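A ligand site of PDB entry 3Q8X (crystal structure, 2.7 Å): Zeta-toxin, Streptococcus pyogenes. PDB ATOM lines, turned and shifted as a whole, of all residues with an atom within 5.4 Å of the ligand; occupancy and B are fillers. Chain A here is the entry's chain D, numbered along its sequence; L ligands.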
ATOM      1  N   LEU A  37      19.117  34.908  33.592  1.00  0.00           N
ATOM      2  CA  LEU A  37      19.109  33.746  32.707  1.00  0.00           C
ATOM      3  C   LEU A  37      18.180  32.669  33.258  1.00  0.00           C
ATOM      4  O   LEU A  37      18.305  32.283  34.412  1.00  0.00           O
ATOM      5  CB  LEU A  37      20.520  33.203  32.440  1.00  0.00           C
ATOM      6  CG  LEU A  37      21.688  34.171  32.207  1.00  0.00           C
ATOM      7  CD1 LEU A  37      22.869  33.453  31.553  1.00  0.00           C
ATOM      8  CD2 LEU A  37      21.314  35.408  31.396  1.00  0.00           C
ATOM      9  N   PRO A  42      11.728  21.345  30.357  1.00  0.00           N
ATOM     10  CA  PRO A  42      10.467  21.635  29.651  1.00  0.00           C
ATOM     11  C   PRO A  42       9.262  21.182  30.466  1.00  0.00           C
ATOM     12  O   PRO A  42       9.303  20.105  31.079  1.00  0.00           O
ATOM     13  CB  PRO A  42      10.581  20.793  28.373  1.00  0.00           C
ATOM     14  CG  PRO A  42      12.046  20.645  28.157  1.00  0.00           C
ATOM     15  CD  PRO A  42      12.650  20.551  29.524  1.00  0.00           C
ATOM     16  N   LYS A  46       8.447  27.874  33.308  1.00  0.00           N
ATOM     17  CA  LYS A  46       9.398  28.985  33.505  1.00  0.00           C
ATOM     18  C   LYS A  46       8.754  30.368  33.348  1.00  0.00           C
ATOM     19  O   LYS A  46       9.377  31.381  33.656  1.00  0.00           O
ATOM     20  CB  LYS A  46      10.628  28.860  32.586  1.00  0.00           C
ATOM     21  CG  LYS A  46      11.321  27.540  32.620  1.00  0.00           C
ATOM     22  CD  LYS A  46      12.402  27.481  31.566  1.00  0.00           C
ATOM     23  CE  LYS A  46      12.213  26.277  30.652  1.00  0.00           C
ATOM     24  NZ  LYS A  46      12.825  26.531  29.315  1.00  0.00           N
ATOM     25  N   ASP A  65      13.182  35.257  23.921  1.00  0.00           N
ATOM     26  CA  ASP A  65      12.727  33.865  23.875  1.00  0.00           C
ATOM     27  C   ASP A  65      12.973  33.236  22.494  1.00  0.00           C
ATOM     28  O   ASP A  65      12.226  33.503  21.550  1.00  0.00           O
ATOM     29  CB  ASP A  65      11.233  33.815  24.289  1.00  0.00           C
ATOM     30  CG  ASP A  65      10.638  32.387  24.319  1.00  0.00           C
ATOM     31  OD1 ASP A  65      11.351  31.365  24.132  1.00  0.00           O
ATOM     32  OD2 ASP A  65       9.403  32.310  24.525  1.00  0.00           O
ATOM     33  N   ASN A  66      14.000  32.402  22.403  1.00  0.00           N
ATOM     34  CA  ASN A  66      14.443  31.798  21.139  1.00  0.00           C
ATOM     35  C   ASN A  66      13.287  31.218  20.291  1.00  0.00           C
ATOM     36  O   ASN A  66      13.273  31.365  19.079  1.00  0.00           O
ATOM     37  CB  ASN A  66      15.525  30.732  21.409  1.00  0.00           C
ATOM     38  CG  ASN A  66      16.295  30.313  20.145  1.00  0.00           C
ATOM     39  OD1 ASN A  66      15.839  30.507  19.020  1.00  0.00           O
ATOM     40  ND2 ASN A  66      17.463  29.715  20.333  1.00  0.00           N
ATOM     41  N   ASP A  67      12.321  30.589  20.963  1.00  0.00           N
ATOM     42  CA  ASP A  67      11.167  29.976  20.312  1.00  0.00           C
ATOM     43  C   ASP A  67      10.330  30.926  19.473  1.00  0.00           C
ATOM     44  O   ASP A  67       9.804  30.529  18.421  1.00  0.00           O
ATOM     45  CB  ASP A  67      10.256  29.341  21.371  1.00  0.00           C
ATOM     46  CG  ASP A  67      10.448  27.837  21.496  1.00  0.00           C
ATOM     47  OD1 ASP A  67      11.580  27.347  21.241  1.00  0.00           O
ATOM     48  OD2 ASP A  67       9.451  27.150  21.857  1.00  0.00           O
ATOM     49  N   LYS A  70      11.223  31.056  15.720  1.00  0.00           N
ATOM     50  CA  LYS A  70      11.146  29.860  14.870  1.00  0.00           C
ATOM     51  C   LYS A  70      10.345  30.088  13.584  1.00  0.00           C
ATOM     52  O   LYS A  70      10.835  29.818  12.487  1.00  0.00           O
ATOM     53  CB  LYS A  70      10.616  28.658  15.656  1.00  0.00           C
ATOM     54  CG  LYS A  70      11.712  27.827  16.332  1.00  0.00           C
ATOM     55  CD  LYS A  70      11.216  27.135  17.617  1.00  0.00           C
ATOM     56  CE  LYS A  70      12.254  26.144  18.162  1.00  0.00           C
ATOM     57  NZ  LYS A  70      13.615  26.744  18.362  1.00  0.00           N
ATOM     58  N   ASN A  96      18.439  30.756  16.317  1.00  0.00           N
ATOM     59  CA  ASN A  96      19.626  30.906  17.155  1.00  0.00           C
ATOM     60  C   ASN A  96      20.397  32.187  16.802  1.00  0.00           C
ATOM     61  O   ASN A  96      20.754  32.967  17.699  1.00  0.00           O
ATOM     62  CB  ASN A  96      20.537  29.663  17.086  1.00  0.00           C
ATOM     63  CG  ASN A  96      19.976  28.453  17.847  1.00  0.00           C
ATOM     64  OD1 ASN A  96      18.966  28.539  18.549  1.00  0.00           O
ATOM     65  ND2 ASN A  96      20.631  27.313  17.685  1.00  0.00           N
ATOM     66  N   THR A  99      18.273  35.381  17.993  1.00  0.00           N
ATOM     67  CA  THR A  99      18.398  35.534  19.445  1.00  0.00           C
ATOM     68  C   THR A  99      19.725  36.164  19.841  1.00  0.00           C
ATOM     69  O   THR A  99      19.755  37.107  20.627  1.00  0.00           O
ATOM     70  CB  THR A  99      18.248  34.170  20.141  1.00  0.00           C
ATOM     71  OG1 THR A  99      17.015  33.571  19.727  1.00  0.00           O
ATOM     72  CG2 THR A  99      18.243  34.335  21.636  1.00  0.00           C
ATOM     73  N   GLU A 100      20.810  35.650  19.260  1.00  0.00           N
ATOM     74  CA  GLU A 100      22.153  36.154  19.539  1.00  0.00           C
ATOM     75  C   GLU A 100      22.408  37.573  19.020  1.00  0.00           C
ATOM     76  O   GLU A 100      23.238  38.290  19.551  1.00  0.00           O
ATOM     77  CB  GLU A 100      23.215  35.195  18.997  1.00  0.00           C
ATOM     78  CG  GLU A 100      23.259  33.835  19.700  1.00  0.00           C
ATOM     79  CD  GLU A 100      24.084  32.810  18.928  1.00  0.00           C
ATOM     80  OE1 GLU A 100      24.915  33.212  18.071  1.00  0.00           O
ATOM     81  OE2 GLU A 100      23.917  31.596  19.205  1.00  0.00           O
ATOM     82  N   ILE A 103      20.077  39.631  21.740  1.00  0.00           N
ATOM     83  CA  ILE A 103      20.868  39.684  22.973  1.00  0.00           C
ATOM     84  C   ILE A 103      22.035  40.642  22.797  1.00  0.00           C
ATOM     85  O   ILE A 103      22.341  41.417  23.702  1.00  0.00           O
ATOM     86  CB  ILE A 103      21.404  38.297  23.412  1.00  0.00           C
ATOM     87  CG1 ILE A 103      20.263  37.366  23.846  1.00  0.00           C
ATOM     88  CG2 ILE A 103      22.389  38.437  24.567  1.00  0.00           C
ATOM     89  CD1 ILE A 103      20.649  35.906  23.925  1.00  0.00           C
ATOM     90  N   ILE A 115      16.519  36.182  29.702  1.00  0.00           N
ATOM     91  CA  ILE A 115      16.908  35.303  28.624  1.00  0.00           C
ATOM     92  C   ILE A 115      16.414  33.869  28.875  1.00  0.00           C
ATOM     93  O   ILE A 115      16.850  33.192  29.819  1.00  0.00           O
ATOM     94  CB  ILE A 115      18.437  35.308  28.372  1.00  0.00           C
ATOM     95  CG1 ILE A 115      18.920  36.730  28.078  1.00  0.00           C
ATOM     96  CG2 ILE A 115      18.785  34.374  27.214  1.00  0.00           C
ATOM     97  CD1 ILE A 115      20.437  36.874  28.024  1.00  0.00           C
ATOM     98  N   GLU A 116      15.511  33.435  28.005  1.00  0.00           N
ATOM     99  CA  GLU A 116      14.888  32.118  28.087  1.00  0.00           C
ATOM    100  C   GLU A 116      15.902  31.005  27.845  1.00  0.00           C
ATOM    101  O   GLU A 116      16.578  30.993  26.820  1.00  0.00           O
ATOM    102  CB  GLU A 116      13.743  32.032  27.063  1.00  0.00           C
ATOM    103  CG  GLU A 116      12.836  30.818  27.207  1.00  0.00           C
ATOM    104  CD  GLU A 116      12.030  30.845  28.483  1.00  0.00           C
ATOM    105  OE1 GLU A 116      11.134  31.719  28.630  1.00  0.00           O
ATOM    106  OE2 GLU A 116      12.314  29.980  29.335  1.00  0.00           O
ATOM    107  N   GLY A 117      15.995  30.080  28.806  1.00  0.00           N
ATOM    108  CA  GLY A 117      16.907  28.940  28.726  1.00  0.00           C
ATOM    109  C   GLY A 117      16.407  27.757  29.554  1.00  0.00           C
ATOM    110  O   GLY A 117      15.514  27.910  30.389  1.00  0.00           O
ATOM    111  N   THR A 118      16.982  26.582  29.327  1.00  0.00           N
ATOM    112  CA  THR A 118      16.584  25.397  30.088  1.00  0.00           C
ATOM    113  C   THR A 118      17.603  24.993  31.141  1.00  0.00           C
ATOM    114  O   THR A 118      17.252  24.385  32.169  1.00  0.00           O
ATOM    115  CB  THR A 118      16.378  24.179  29.169  1.00  0.00           C
ATOM    116  OG1 THR A 118      17.642  23.816  28.599  1.00  0.00           O
ATOM    117  CG2 THR A 118      15.339  24.459  28.076  1.00  0.00           C
ATOM    118  N   GLY A 119      18.864  25.318  30.887  1.00  0.00           N
ATOM    119  CA  GLY A 119      19.979  24.918  31.731  1.00  0.00           C
ATOM    120  C   GLY A 119      20.464  23.514  31.428  1.00  0.00           C
ATOM    121  O   GLY A 119      21.100  22.878  32.267  1.00  0.00           O
ATOM    122  N   ARG A 120      20.169  23.016  30.229  1.00  0.00           N
ATOM    123  CA  ARG A 120      20.627  21.701  29.796  1.00  0.00           C
ATOM    124  C   ARG A 120      22.165  21.639  29.780  1.00  0.00           C
ATOM    125  O   ARG A 120      22.766  20.630  30.122  1.00  0.00           O
ATOM    126  CB  ARG A 120      20.044  21.360  28.420  1.00  0.00           C
ATOM    127  CG  ARG A 120      20.608  20.120  27.742  1.00  0.00           C
ATOM    128  CD  ARG A 120      20.029  19.900  26.344  1.00  0.00           C
ATOM    129  NE  ARG A 120      19.928  21.137  25.556  1.00  0.00           N
ATOM    130  CZ  ARG A 120      20.840  21.578  24.698  1.00  0.00           C
ATOM    131  NH1 ARG A 120      21.965  20.901  24.488  1.00  0.00           N
ATOM    132  NH2 ARG A 120      20.630  22.714  24.038  1.00  0.00           N
ATOM    133  N   THR A 121      22.778  22.770  29.419  1.00  0.00           N
ATOM    134  CA  THR A 121      24.235  22.910  29.294  1.00  0.00           C
ATOM    135  C   THR A 121      24.798  23.950  30.255  1.00  0.00           C
ATOM    136  O   THR A 121      24.125  24.914  30.602  1.00  0.00           O
ATOM    137  CB  THR A 121      24.611  23.414  27.898  1.00  0.00           C
ATOM    138  OG1 THR A 121      23.822  24.576  27.587  1.00  0.00           O
ATOM    139  CG2 THR A 121      24.388  22.337  26.839  1.00  0.00           C
ATOM    140  N   VAL A 124      26.275  27.296  27.502  1.00  0.00           N
ATOM    141  CA  VAL A 124      25.479  28.435  27.046  1.00  0.00           C
ATOM    142  C   VAL A 124      25.353  29.567  28.077  1.00  0.00           C
ATOM    143  O   VAL A 124      25.754  30.705  27.785  1.00  0.00           O
ATOM    144  CB  VAL A 124      24.099  27.970  26.460  1.00  0.00           C
ATOM    145  CG1 VAL A 124      23.130  29.121  26.348  1.00  0.00           C
ATOM    146  CG2 VAL A 124      24.294  27.316  25.112  1.00  0.00           C
ATOM    147  N   PRO A 125      24.808  29.275  29.292  1.00  0.00           N
ATOM    148  CA  PRO A 125      24.726  30.344  30.303  1.00  0.00           C
ATOM    149  C   PRO A 125      26.090  30.955  30.670  1.00  0.00           C
ATOM    150  O   PRO A 125      26.183  32.175  30.736  1.00  0.00           O
ATOM    151  CB  PRO A 125      24.074  29.643  31.517  1.00  0.00           C
ATOM    152  CG  PRO A 125      24.252  28.187  31.283  1.00  0.00           C
ATOM    153  CD  PRO A 125      24.242  28.008  29.796  1.00  0.00           C
ATOM    154  N   THR A 128      27.087  33.096  27.933  1.00  0.00           N
ATOM    155  CA  THR A 128      26.241  34.287  27.914  1.00  0.00           C
ATOM    156  C   THR A 128      26.606  35.245  29.047  1.00  0.00           C
ATOM    157  O   THR A 128      26.747  36.456  28.817  1.00  0.00           O
ATOM    158  CB  THR A 128      24.744  33.920  28.020  1.00  0.00           C
ATOM    159  OG1 THR A 128      24.432  32.904  27.074  1.00  0.00           O
ATOM    160  CG2 THR A 128      23.874  35.125  27.725  1.00  0.00           C
ATOM    161  N   ARG A 171       3.563  19.883  18.126  1.00  0.00           N
ATOM    162  CA  ARG A 171       4.563  18.805  18.192  1.00  0.00           C
ATOM    163  C   ARG A 171       5.040  18.672  19.638  1.00  0.00           C
ATOM    164  O   ARG A 171       5.427  19.661  20.281  1.00  0.00           O
ATOM    165  CB  ARG A 171       5.736  19.090  17.256  1.00  0.00           C
ATOM    166  CG  ARG A 171       6.628  17.868  16.983  1.00  0.00           C
ATOM    167  CD  ARG A 171       7.962  18.257  16.337  1.00  0.00           C
ATOM    168  NE  ARG A 171       8.564  19.437  16.969  1.00  0.00           N
ATOM    169  CZ  ARG A 171       9.451  19.405  17.969  1.00  0.00           C
ATOM    170  NH1 ARG A 171       9.861  18.242  18.474  1.00  0.00           N
ATOM    171  NH2 ARG A 171       9.927  20.537  18.463  1.00  0.00           N
ATOM    172  N   THR A 173       7.090  17.506  23.155  1.00  0.00           N
ATOM    173  CA  THR A 173       8.463  17.420  23.636  1.00  0.00           C
ATOM    174  C   THR A 173       8.784  15.938  23.830  1.00  0.00           C
ATOM    175  O   THR A 173       8.064  15.249  24.552  1.00  0.00           O
ATOM    176  CB  THR A 173       8.669  18.181  24.978  1.00  0.00           C
ATOM    177  OG1 THR A 173       8.258  19.551  24.835  1.00  0.00           O
ATOM    178  CG2 THR A 173      10.137  18.140  25.407  1.00  0.00           C
HETATM  179  C1  LIG L   1      15.379  24.899  23.155  1.00  0.00           C
HETATM  180  C2  LIG L   1      14.219  25.837  23.508  1.00  0.00           C
HETATM  181  C3  LIG L   1      12.943  25.079  23.931  1.00  0.00           C
HETATM  182  C4  LIG L   1      12.624  23.923  22.986  1.00  0.00           C
HETATM  183  C5  LIG L   1      13.875  23.095  22.682  1.00  0.00           C
HETATM  184  C6  LIG L   1      13.645  21.993  21.664  1.00  0.00           C
HETATM  185  C7  LIG L   1      14.740  28.067  24.271  1.00  0.00           C
HETATM  186  C8  LIG L   1      13.538  28.880  24.680  1.00  0.00           C
HETATM  187  N1  LIG L   1      14.648  26.769  24.534  1.00  0.00           N
HETATM  188  O1  LIG L   1      15.905  24.271  24.329  1.00  0.00           O
HETATM  189  O2  LIG L   1      11.841  26.003  23.957  1.00  0.00           O
HETATM  190  O3  LIG L   1      11.600  23.090  23.557  1.00  0.00           O
HETATM  191  O4  LIG L   1      14.938  23.936  22.199  1.00  0.00           O
HETATM  192  O5  LIG L   1      14.726  21.052  21.784  1.00  0.00           O
HETATM  193  O6  LIG L   1      15.721  28.551  23.717  1.00  0.00           O
HETATM  194  N2  LIG L   1      20.442  31.222  24.011  1.00  0.00           N
HETATM  195  C9  LIG L   1      21.414  32.235  24.245  1.00  0.00           C
HETATM  196  N3  LIG L   1      21.737  32.573  25.501  1.00  0.00           N
HETATM  197  C10 LIG L   1      21.172  31.964  26.553  1.00  0.00           C
HETATM  198  C11 LIG L   1      20.208  30.968  26.371  1.00  0.00           C
HETATM  199  C12 LIG L   1      19.868  30.608  25.065  1.00  0.00           C
HETATM  200  O7  LIG L   1      21.977  32.820  23.283  1.00  0.00           O
HETATM  201  O8  LIG L   1      21.483  32.306  27.718  1.00  0.00           O
HETATM  202  C13 LIG L   1      20.103  30.812  22.642  1.00  0.00           C
HETATM  203  C14 LIG L   1      21.358  30.132  22.110  1.00  0.00           C
HETATM  204  O9  LIG L   1      21.471  30.310  20.688  1.00  0.00           O
HETATM  205  C15 LIG L   1      21.149  28.679  22.524  1.00  0.00           C
HETATM  206  C16 LIG L   1      19.654  28.515  22.299  1.00  0.00           C
HETATM  207  O10 LIG L   1      19.077  29.798  22.610  1.00  0.00           O
HETATM  208  O11 LIG L   1      21.961  27.736  21.828  1.00  0.00           O
HETATM  209  C17 LIG L   1      19.037  27.419  23.168  1.00  0.00           C
HETATM  210  O12 LIG L   1      19.192  27.749  24.549  1.00  0.00           O
HETATM  211  P1  LIG L   1      18.966  26.636  25.674  1.00  0.00           P
HETATM  212  O13 LIG L   1      18.717  27.355  26.965  1.00  0.00           O
HETATM  213  O14 LIG L   1      20.100  25.638  25.570  1.00  0.00           O
HETATM  214  O15 LIG L   1      17.586  25.934  25.220  1.00  0.00           O
HETATM  215  P2  LIG L   1      17.477  24.412  24.683  1.00  0.00           P
HETATM  216  O16 LIG L   1      18.271  24.305  23.400  1.00  0.00           O
HETATM  217  O17 LIG L   1      17.763  23.459  25.835  1.00  0.00           O
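Merely in contact with the ligand: Asp 65, Asn 96, Ile 103, Ile 115, Glu 116, Gly 117 and Val 124.
NH2 of Arg 120 lies within salt-bridge range of O16 of the ligand. The side-chain carboxylate (OD1) of Asp 67 lies within hydrogen-bond range of an oxygen (O2) of the ligand. The side-chain carboxylate (OE2) of Glu 100 is in hydrogen-bond range of an oxygen (O9) of the ligand (3.1 Å). An oxygen (O13) of the ligand sits at hydrogen-bond distance from the backbone NH (N) of Thr 118, 3.0 Å away. O17 of the ligand sits at hydrogen-bond distance from OG1 of Thr 118. An oxygen (O10) of the ligand sits at hydrogen-bond distance from the side-chain amide nitrogen of Asn 66. The side-chain hydroxyl (OG1) of Thr 128 is in hydrogen-bond range of an oxygen (O8) of the ligand (3.1 Å).
ND2 of Asn 66 lies within hydrogen-bond range of OD1 of Asn 96 (2.6 Å). OD1 of Asp 67 is in salt-bridge range of NZ of Lys 70 (3.6 Å). The side-chain amide oxygen (OD1) of Asn 66 sits at hydrogen-bond distance from the side-chain hydroxyl (OG1) of Thr 99, at 3.4 Å. The side-chain amino group (NZ) of Lys 46 sits at hydrogen-bond distance from the backbone carbonyl oxygen (O) of Gly 117. The side-chain hydroxyl (OG1) of Thr 118 sits at hydrogen-bond distance from the backbone NH (N) of Arg 120 (3.1 Å). N of Asp 67 sits close to OD1 of Asp 65 (3.4 Å). The side-chain amino group (NZ) of Lys 46 lies within salt-bridge range of the side-chain carboxylate (OE2) of Glu 116 (3.5 Å). OG1 of Thr 128 sits at hydrogen-bond distance from O of Val 124, 2.7 Å away.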
